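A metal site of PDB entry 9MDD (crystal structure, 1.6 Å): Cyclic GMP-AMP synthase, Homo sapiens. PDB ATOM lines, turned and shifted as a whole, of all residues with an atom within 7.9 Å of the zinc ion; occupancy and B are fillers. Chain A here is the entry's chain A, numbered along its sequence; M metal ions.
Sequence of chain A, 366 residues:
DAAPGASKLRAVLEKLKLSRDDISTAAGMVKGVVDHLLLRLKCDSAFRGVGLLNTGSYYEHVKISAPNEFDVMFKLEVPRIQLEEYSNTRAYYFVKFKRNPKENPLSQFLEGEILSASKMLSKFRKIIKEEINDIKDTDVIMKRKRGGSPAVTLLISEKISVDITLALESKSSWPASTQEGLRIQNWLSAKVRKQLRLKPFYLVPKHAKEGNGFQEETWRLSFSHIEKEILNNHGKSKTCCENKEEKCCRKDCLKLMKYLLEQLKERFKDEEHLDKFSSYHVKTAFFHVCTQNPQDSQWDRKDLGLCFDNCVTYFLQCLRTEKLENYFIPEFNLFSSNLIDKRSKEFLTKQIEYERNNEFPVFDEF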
ATOM      1  N   LEU A 231     -19.668   3.066 -11.332  1.00  0.00           N
ATOM      2  CA  LEU A 231     -20.984   3.676 -11.075  1.00  0.00           C
ATOM      3  C   LEU A 231     -22.122   2.661 -11.170  1.00  0.00           C
ATOM      4  O   LEU A 231     -23.142   2.823 -10.469  1.00  0.00           O
ATOM      5  CB  LEU A 231     -21.245   4.845 -12.025  1.00  0.00           C
ATOM      6  CG  LEU A 231     -20.562   6.115 -11.491  1.00  0.00           C
ATOM      7  CD1 LEU A 231     -20.427   7.186 -12.544  1.00  0.00           C
ATOM      8  CD2 LEU A 231     -21.345   6.689 -10.269  1.00  0.00           C
ATOM      9  N   ASN A 233     -21.914  -0.535 -10.373  1.00  0.00           N
ATOM     10  CA  ASN A 233     -21.720  -1.551  -9.335  1.00  0.00           C
ATOM     11  C   ASN A 233     -21.045  -0.841  -8.173  1.00  0.00           C
ATOM     12  O   ASN A 233     -19.888  -1.074  -7.848  1.00  0.00           O
ATOM     13  CB  ASN A 233     -20.891  -2.735  -9.827  1.00  0.00           C
ATOM     14  CG  ASN A 233     -21.136  -3.993  -9.036  1.00  0.00           C
ATOM     15  OD1 ASN A 233     -21.874  -3.991  -8.036  1.00  0.00           O
ATOM     16  ND2 ASN A 233     -20.538  -5.105  -9.484  1.00  0.00           N
ATOM     17  N   HIS A 234     -21.815   0.034  -7.522  1.00  0.00           N
ATOM     18  CA  HIS A 234     -21.246   1.136  -6.758  1.00  0.00           C
ATOM     19  C   HIS A 234     -21.274   0.940  -5.245  1.00  0.00           C
ATOM     20  O   HIS A 234     -20.791   1.811  -4.512  1.00  0.00           O
ATOM     21  CB  HIS A 234     -21.986   2.439  -7.092  1.00  0.00           C
ATOM     22  CG  HIS A 234     -23.433   2.388  -6.718  1.00  0.00           C
ATOM     23  ND1 HIS A 234     -24.444   2.362  -7.649  1.00  0.00           N
ATOM     24  CD2 HIS A 234     -24.020   2.262  -5.503  1.00  0.00           C
ATOM     25  CE1 HIS A 234     -25.611   2.262  -7.027  1.00  0.00           C
ATOM     26  NE2 HIS A 234     -25.380   2.184  -5.729  1.00  0.00           N
ATOM     27  N   GLY A 235     -21.839  -0.158  -4.757  1.00  0.00           N
ATOM     28  CA  GLY A 235     -22.050  -0.301  -3.331  1.00  0.00           C
ATOM     29  C   GLY A 235     -20.999  -1.203  -2.710  1.00  0.00           C
ATOM     30  O   GLY A 235     -20.387  -2.031  -3.381  1.00  0.00           O
ATOM     31  N   LYS A 236     -20.793  -1.047  -1.394  1.00  0.00           N
ATOM     32  CA  LYS A 236     -20.052  -2.090  -0.683  1.00  0.00           C
ATOM     33  C   LYS A 236     -20.829  -3.411  -0.720  1.00  0.00           C
ATOM     34  O   LYS A 236     -20.246  -4.480  -0.953  1.00  0.00           O
ATOM     35  CB  LYS A 236     -19.770  -1.674   0.763  1.00  0.00           C
ATOM     36  CG  LYS A 236     -19.070  -2.812   1.548  1.00  0.00           C
ATOM     37  CD  LYS A 236     -18.559  -2.343   2.917  1.00  0.00           C
ATOM     38  CE  LYS A 236     -17.386  -1.397   2.778  1.00  0.00           C
ATOM     39  NZ  LYS A 236     -16.237  -2.045   2.066  1.00  0.00           N
ATOM     40  N   SER A 237     -22.134  -3.352  -0.462  1.00  0.00           N
ATOM     41  CA  SER A 237     -23.016  -4.503  -0.673  1.00  0.00           C
ATOM     42  C   SER A 237     -23.219  -4.744  -2.166  1.00  0.00           C
ATOM     43  O   SER A 237     -23.520  -3.816  -2.914  1.00  0.00           O
ATOM     44  CB  SER A 237     -24.372  -4.269  -0.026  1.00  0.00           C
ATOM     45  OG  SER A 237     -25.263  -5.315  -0.424  1.00  0.00           O
ATOM     46  N   THR A 239     -25.724  -6.074  -3.338  1.00  0.00           N
ATOM     47  CA  THR A 239     -27.127  -5.831  -3.620  1.00  0.00           C
ATOM     48  C   THR A 239     -27.527  -4.380  -3.346  1.00  0.00           C
ATOM     49  O   THR A 239     -28.720  -4.079  -3.271  1.00  0.00           O
ATOM     50  CB  THR A 239     -28.037  -6.808  -2.857  1.00  0.00           C
ATOM     51  OG1 THR A 239     -27.661  -6.913  -1.472  1.00  0.00           O
ATOM     52  CG2 THR A 239     -27.958  -8.193  -3.499  1.00  0.00           C
ATOM     53  N   CYS A 240     -26.559  -3.467  -3.238  1.00  0.00           N
ATOM     54  CA  CYS A 240     -26.914  -2.057  -3.090  1.00  0.00           C
ATOM     55  C   CYS A 240     -27.815  -1.611  -4.231  1.00  0.00           C
ATOM     56  O   CYS A 240     -27.513  -1.860  -5.397  1.00  0.00           O
ATOM     57  CB  CYS A 240     -25.635  -1.208  -3.039  1.00  0.00           C
ATOM     58  SG  CYS A 240     -25.896   0.520  -2.537  1.00  0.00           S
ATOM     59  N   CYS A 241     -28.929  -0.969  -3.891  1.00  0.00           N
ATOM     60  CA  CYS A 241     -29.910  -0.472  -4.856  1.00  0.00           C
ATOM     61  C   CYS A 241     -30.614  -1.579  -5.650  1.00  0.00           C
ATOM     62  O   CYS A 241     -31.236  -1.299  -6.681  1.00  0.00           O
ATOM     63  CB  CYS A 241     -29.285   0.555  -5.812  1.00  0.00           C
ATOM     64  SG  CYS A 241     -28.842   2.104  -4.948  1.00  0.00           S
ATOM     65  N   GLU A 242     -30.550  -2.824  -5.193  1.00  0.00           N
ATOM     66  CA  GLU A 242     -31.341  -3.899  -5.798  1.00  0.00           C
ATOM     67  C   GLU A 242     -32.594  -4.220  -5.010  1.00  0.00           C
ATOM     68  O   GLU A 242     -33.395  -5.060  -5.458  1.00  0.00           O
ATOM     69  CB  GLU A 242     -30.481  -5.168  -5.956  1.00  0.00           C
ATOM     70  CG  GLU A 242     -29.569  -5.105  -7.157  1.00  0.00           C
ATOM     71  CD  GLU A 242     -28.941  -6.456  -7.521  1.00  0.00           C
ATOM     72  OE1 GLU A 242     -29.272  -7.461  -6.863  1.00  0.00           O
ATOM     73  OE2 GLU A 242     -28.142  -6.489  -8.477  1.00  0.00           O
ATOM     74  N   GLU A 246     -31.978  -1.321   0.594  1.00  0.00           N
ATOM     75  CA  GLU A 246     -30.614  -0.900   0.268  1.00  0.00           C
ATOM     76  C   GLU A 246     -30.591   0.151  -0.825  1.00  0.00           C
ATOM     77  O   GLU A 246     -29.700   0.163  -1.678  1.00  0.00           O
ATOM     78  CB  GLU A 246     -29.747  -2.086  -0.153  1.00  0.00           C
ATOM     79  CG  GLU A 246     -29.542  -3.134   0.898  1.00  0.00           C
ATOM     80  CD  GLU A 246     -28.638  -4.247   0.384  1.00  0.00           C
ATOM     81  OE1 GLU A 246     -27.421  -3.994   0.253  1.00  0.00           O
ATOM     82  OE2 GLU A 246     -29.154  -5.342   0.094  1.00  0.00           O
ATOM     83  N   LYS A 247     -31.568   1.055  -0.851  1.00  0.00           N
ATOM     84  CA  LYS A 247     -31.501   2.158  -1.796  1.00  0.00           C
ATOM     85  C   LYS A 247     -30.597   3.241  -1.214  1.00  0.00           C
ATOM     86  O   LYS A 247     -30.921   3.845  -0.193  1.00  0.00           O
ATOM     87  CB  LYS A 247     -32.901   2.678  -2.126  1.00  0.00           C
ATOM     88  CG  LYS A 247     -33.703   1.723  -2.988  1.00  0.00           C
ATOM     89  CD  LYS A 247     -33.320   1.883  -4.460  1.00  0.00           C
ATOM     90  CE  LYS A 247     -34.103   0.965  -5.380  1.00  0.00           C
ATOM     91  NZ  LYS A 247     -33.943  -0.478  -4.999  1.00  0.00           N
ATOM     92  N   CYS A 248     -29.439   3.432  -1.829  1.00  0.00           N
ATOM     93  CA  CYS A 248     -28.520   4.470  -1.396  1.00  0.00           C
ATOM     94  C   CYS A 248     -28.715   5.726  -2.242  1.00  0.00           C
ATOM     95  O   CYS A 248     -29.450   5.718  -3.233  1.00  0.00           O
ATOM     96  CB  CYS A 248     -27.067   3.969  -1.460  1.00  0.00           C
ATOM     97  SG  CYS A 248     -26.265   4.053  -3.120  1.00  0.00           S
ATOM     98  N   CYS A 249     -28.093   6.820  -1.809  1.00  0.00           N
ATOM     99  CA  CYS A 249     -28.239   8.089  -2.538  1.00  0.00           C
ATOM    100  C   CYS A 249     -26.972   8.509  -3.280  1.00  0.00           C
ATOM    101  O   CYS A 249     -26.847   9.686  -3.655  1.00  0.00           O
ATOM    102  CB  CYS A 249     -28.686   9.200  -1.586  1.00  0.00           C
ATOM    103  SG  CYS A 249     -27.502   9.684  -0.294  1.00  0.00           S
ATOM    104  N   ARG A 250     -26.063   7.571  -3.570  1.00  0.00           N
ATOM    105  CA  ARG A 250     -24.833   7.943  -4.281  1.00  0.00           C
ATOM    106  C   ARG A 250     -25.149   8.575  -5.634  1.00  0.00           C
ATOM    107  O   ARG A 250     -24.680   9.675  -5.929  1.00  0.00           O
ATOM    108  CB  ARG A 250     -23.919   6.722  -4.452  1.00  0.00           C
ATOM    109  CG  ARG A 250     -23.181   6.300  -3.161  1.00  0.00           C
ATOM    110  CD  ARG A 250     -22.187   5.171  -3.479  1.00  0.00           C
ATOM    111  NE  ARG A 250     -21.549   4.590  -2.298  1.00  0.00           N
ATOM    112  CZ  ARG A 250     -22.005   3.536  -1.622  1.00  0.00           C
ATOM    113  NH1 ARG A 250     -23.205   3.024  -1.849  1.00  0.00           N
ATOM    114  NH2 ARG A 250     -21.216   2.964  -0.714  1.00  0.00           N
ATOM    115  N   LYS A 251     -25.929   7.883  -6.478  1.00  0.00           N
ATOM    116  CA  LYS A 251     -26.168   8.450  -7.806  1.00  0.00           C
ATOM    117  C   LYS A 251     -26.984   9.740  -7.746  1.00  0.00           C
ATOM    118  O   LYS A 251     -26.740  10.661  -8.539  1.00  0.00           O
ATOM    119  CB  LYS A 251     -26.829   7.425  -8.715  1.00  0.00           C
ATOM    120  CG  LYS A 251     -25.871   6.334  -9.113  1.00  0.00           C
ATOM    121  CD  LYS A 251     -26.392   5.556 -10.318  1.00  0.00           C
ATOM    122  CE  LYS A 251     -25.357   4.547 -10.750  1.00  0.00           C
ATOM    123  NZ  LYS A 251     -25.790   3.732 -11.921  1.00  0.00           N
ATOM    124  N   ASP A 296     -22.126   1.672   2.744  1.00  0.00           N
ATOM    125  CA  ASP A 296     -23.446   2.031   2.199  1.00  0.00           C
ATOM    126  C   ASP A 296     -24.265   2.813   3.220  1.00  0.00           C
ATOM    127  O   ASP A 296     -25.059   3.695   2.851  1.00  0.00           O
ATOM    128  CB  ASP A 296     -24.219   0.785   1.756  1.00  0.00           C
ATOM    129  CG  ASP A 296     -23.516   0.034   0.648  1.00  0.00           C
ATOM    130  OD1 ASP A 296     -22.670   0.666  -0.018  1.00  0.00           O
ATOM    131  OD2 ASP A 296     -23.800  -1.185   0.460  1.00  0.00           O
ATOM    132  N   TRP A 299     -24.569   6.503   2.988  1.00  0.00           N
ATOM    133  CA  TRP A 299     -25.287   7.005   1.828  1.00  0.00           C
ATOM    134  C   TRP A 299     -26.752   6.596   1.878  1.00  0.00           C
ATOM    135  O   TRP A 299     -27.384   6.351   0.845  1.00  0.00           O
ATOM    136  CB  TRP A 299     -24.647   6.493   0.533  1.00  0.00           C
ATOM    137  CG  TRP A 299     -23.241   6.956   0.368  1.00  0.00           C
ATOM    138  CD1 TRP A 299     -22.124   6.302   0.775  1.00  0.00           C
ATOM    139  CD2 TRP A 299     -22.807   8.145  -0.296  1.00  0.00           C
ATOM    140  NE1 TRP A 299     -21.002   7.020   0.430  1.00  0.00           N
ATOM    141  CE2 TRP A 299     -21.395   8.153  -0.242  1.00  0.00           C
ATOM    142  CE3 TRP A 299     -23.476   9.211  -0.917  1.00  0.00           C
ATOM    143  CZ2 TRP A 299     -20.632   9.179  -0.809  1.00  0.00           C
ATOM    144  CZ3 TRP A 299     -22.713  10.236  -1.485  1.00  0.00           C
ATOM    145  CH2 TRP A 299     -21.303  10.210  -1.422  1.00  0.00           C
HETATM  146 ZN    ZN M   1     -26.707   1.975  -4.147  1.00  0.00          ZN
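The zinc ion is bound by NE2 of His 234. The zinc ion is bound by SG of Cys 241, 2.3 Å away. The zinc ion is bound by SG of Cys 240. The zinc ion is bound by SG of Cys 248, at 2.4 Å.
O of Glu 246 sits at hydrogen-bond distance from N of Cys 241. The side-chain sulfur (SG) of Cys 240 lies close to the guanidinium group (NH1) of Arg 250 (3.7 Å). NH1 of Arg 250 lies close to SG of Cys 248 (3.5 Å). ND1 of His 234 sits at hydrogen-bond distance from O of Leu 231, at 3.1 Å. The backbone carbonyl oxygen (O) of Cys 241 lies within hydrogen-bond range of the side-chain amino group (NZ) of Lys 247 (3.3 Å).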
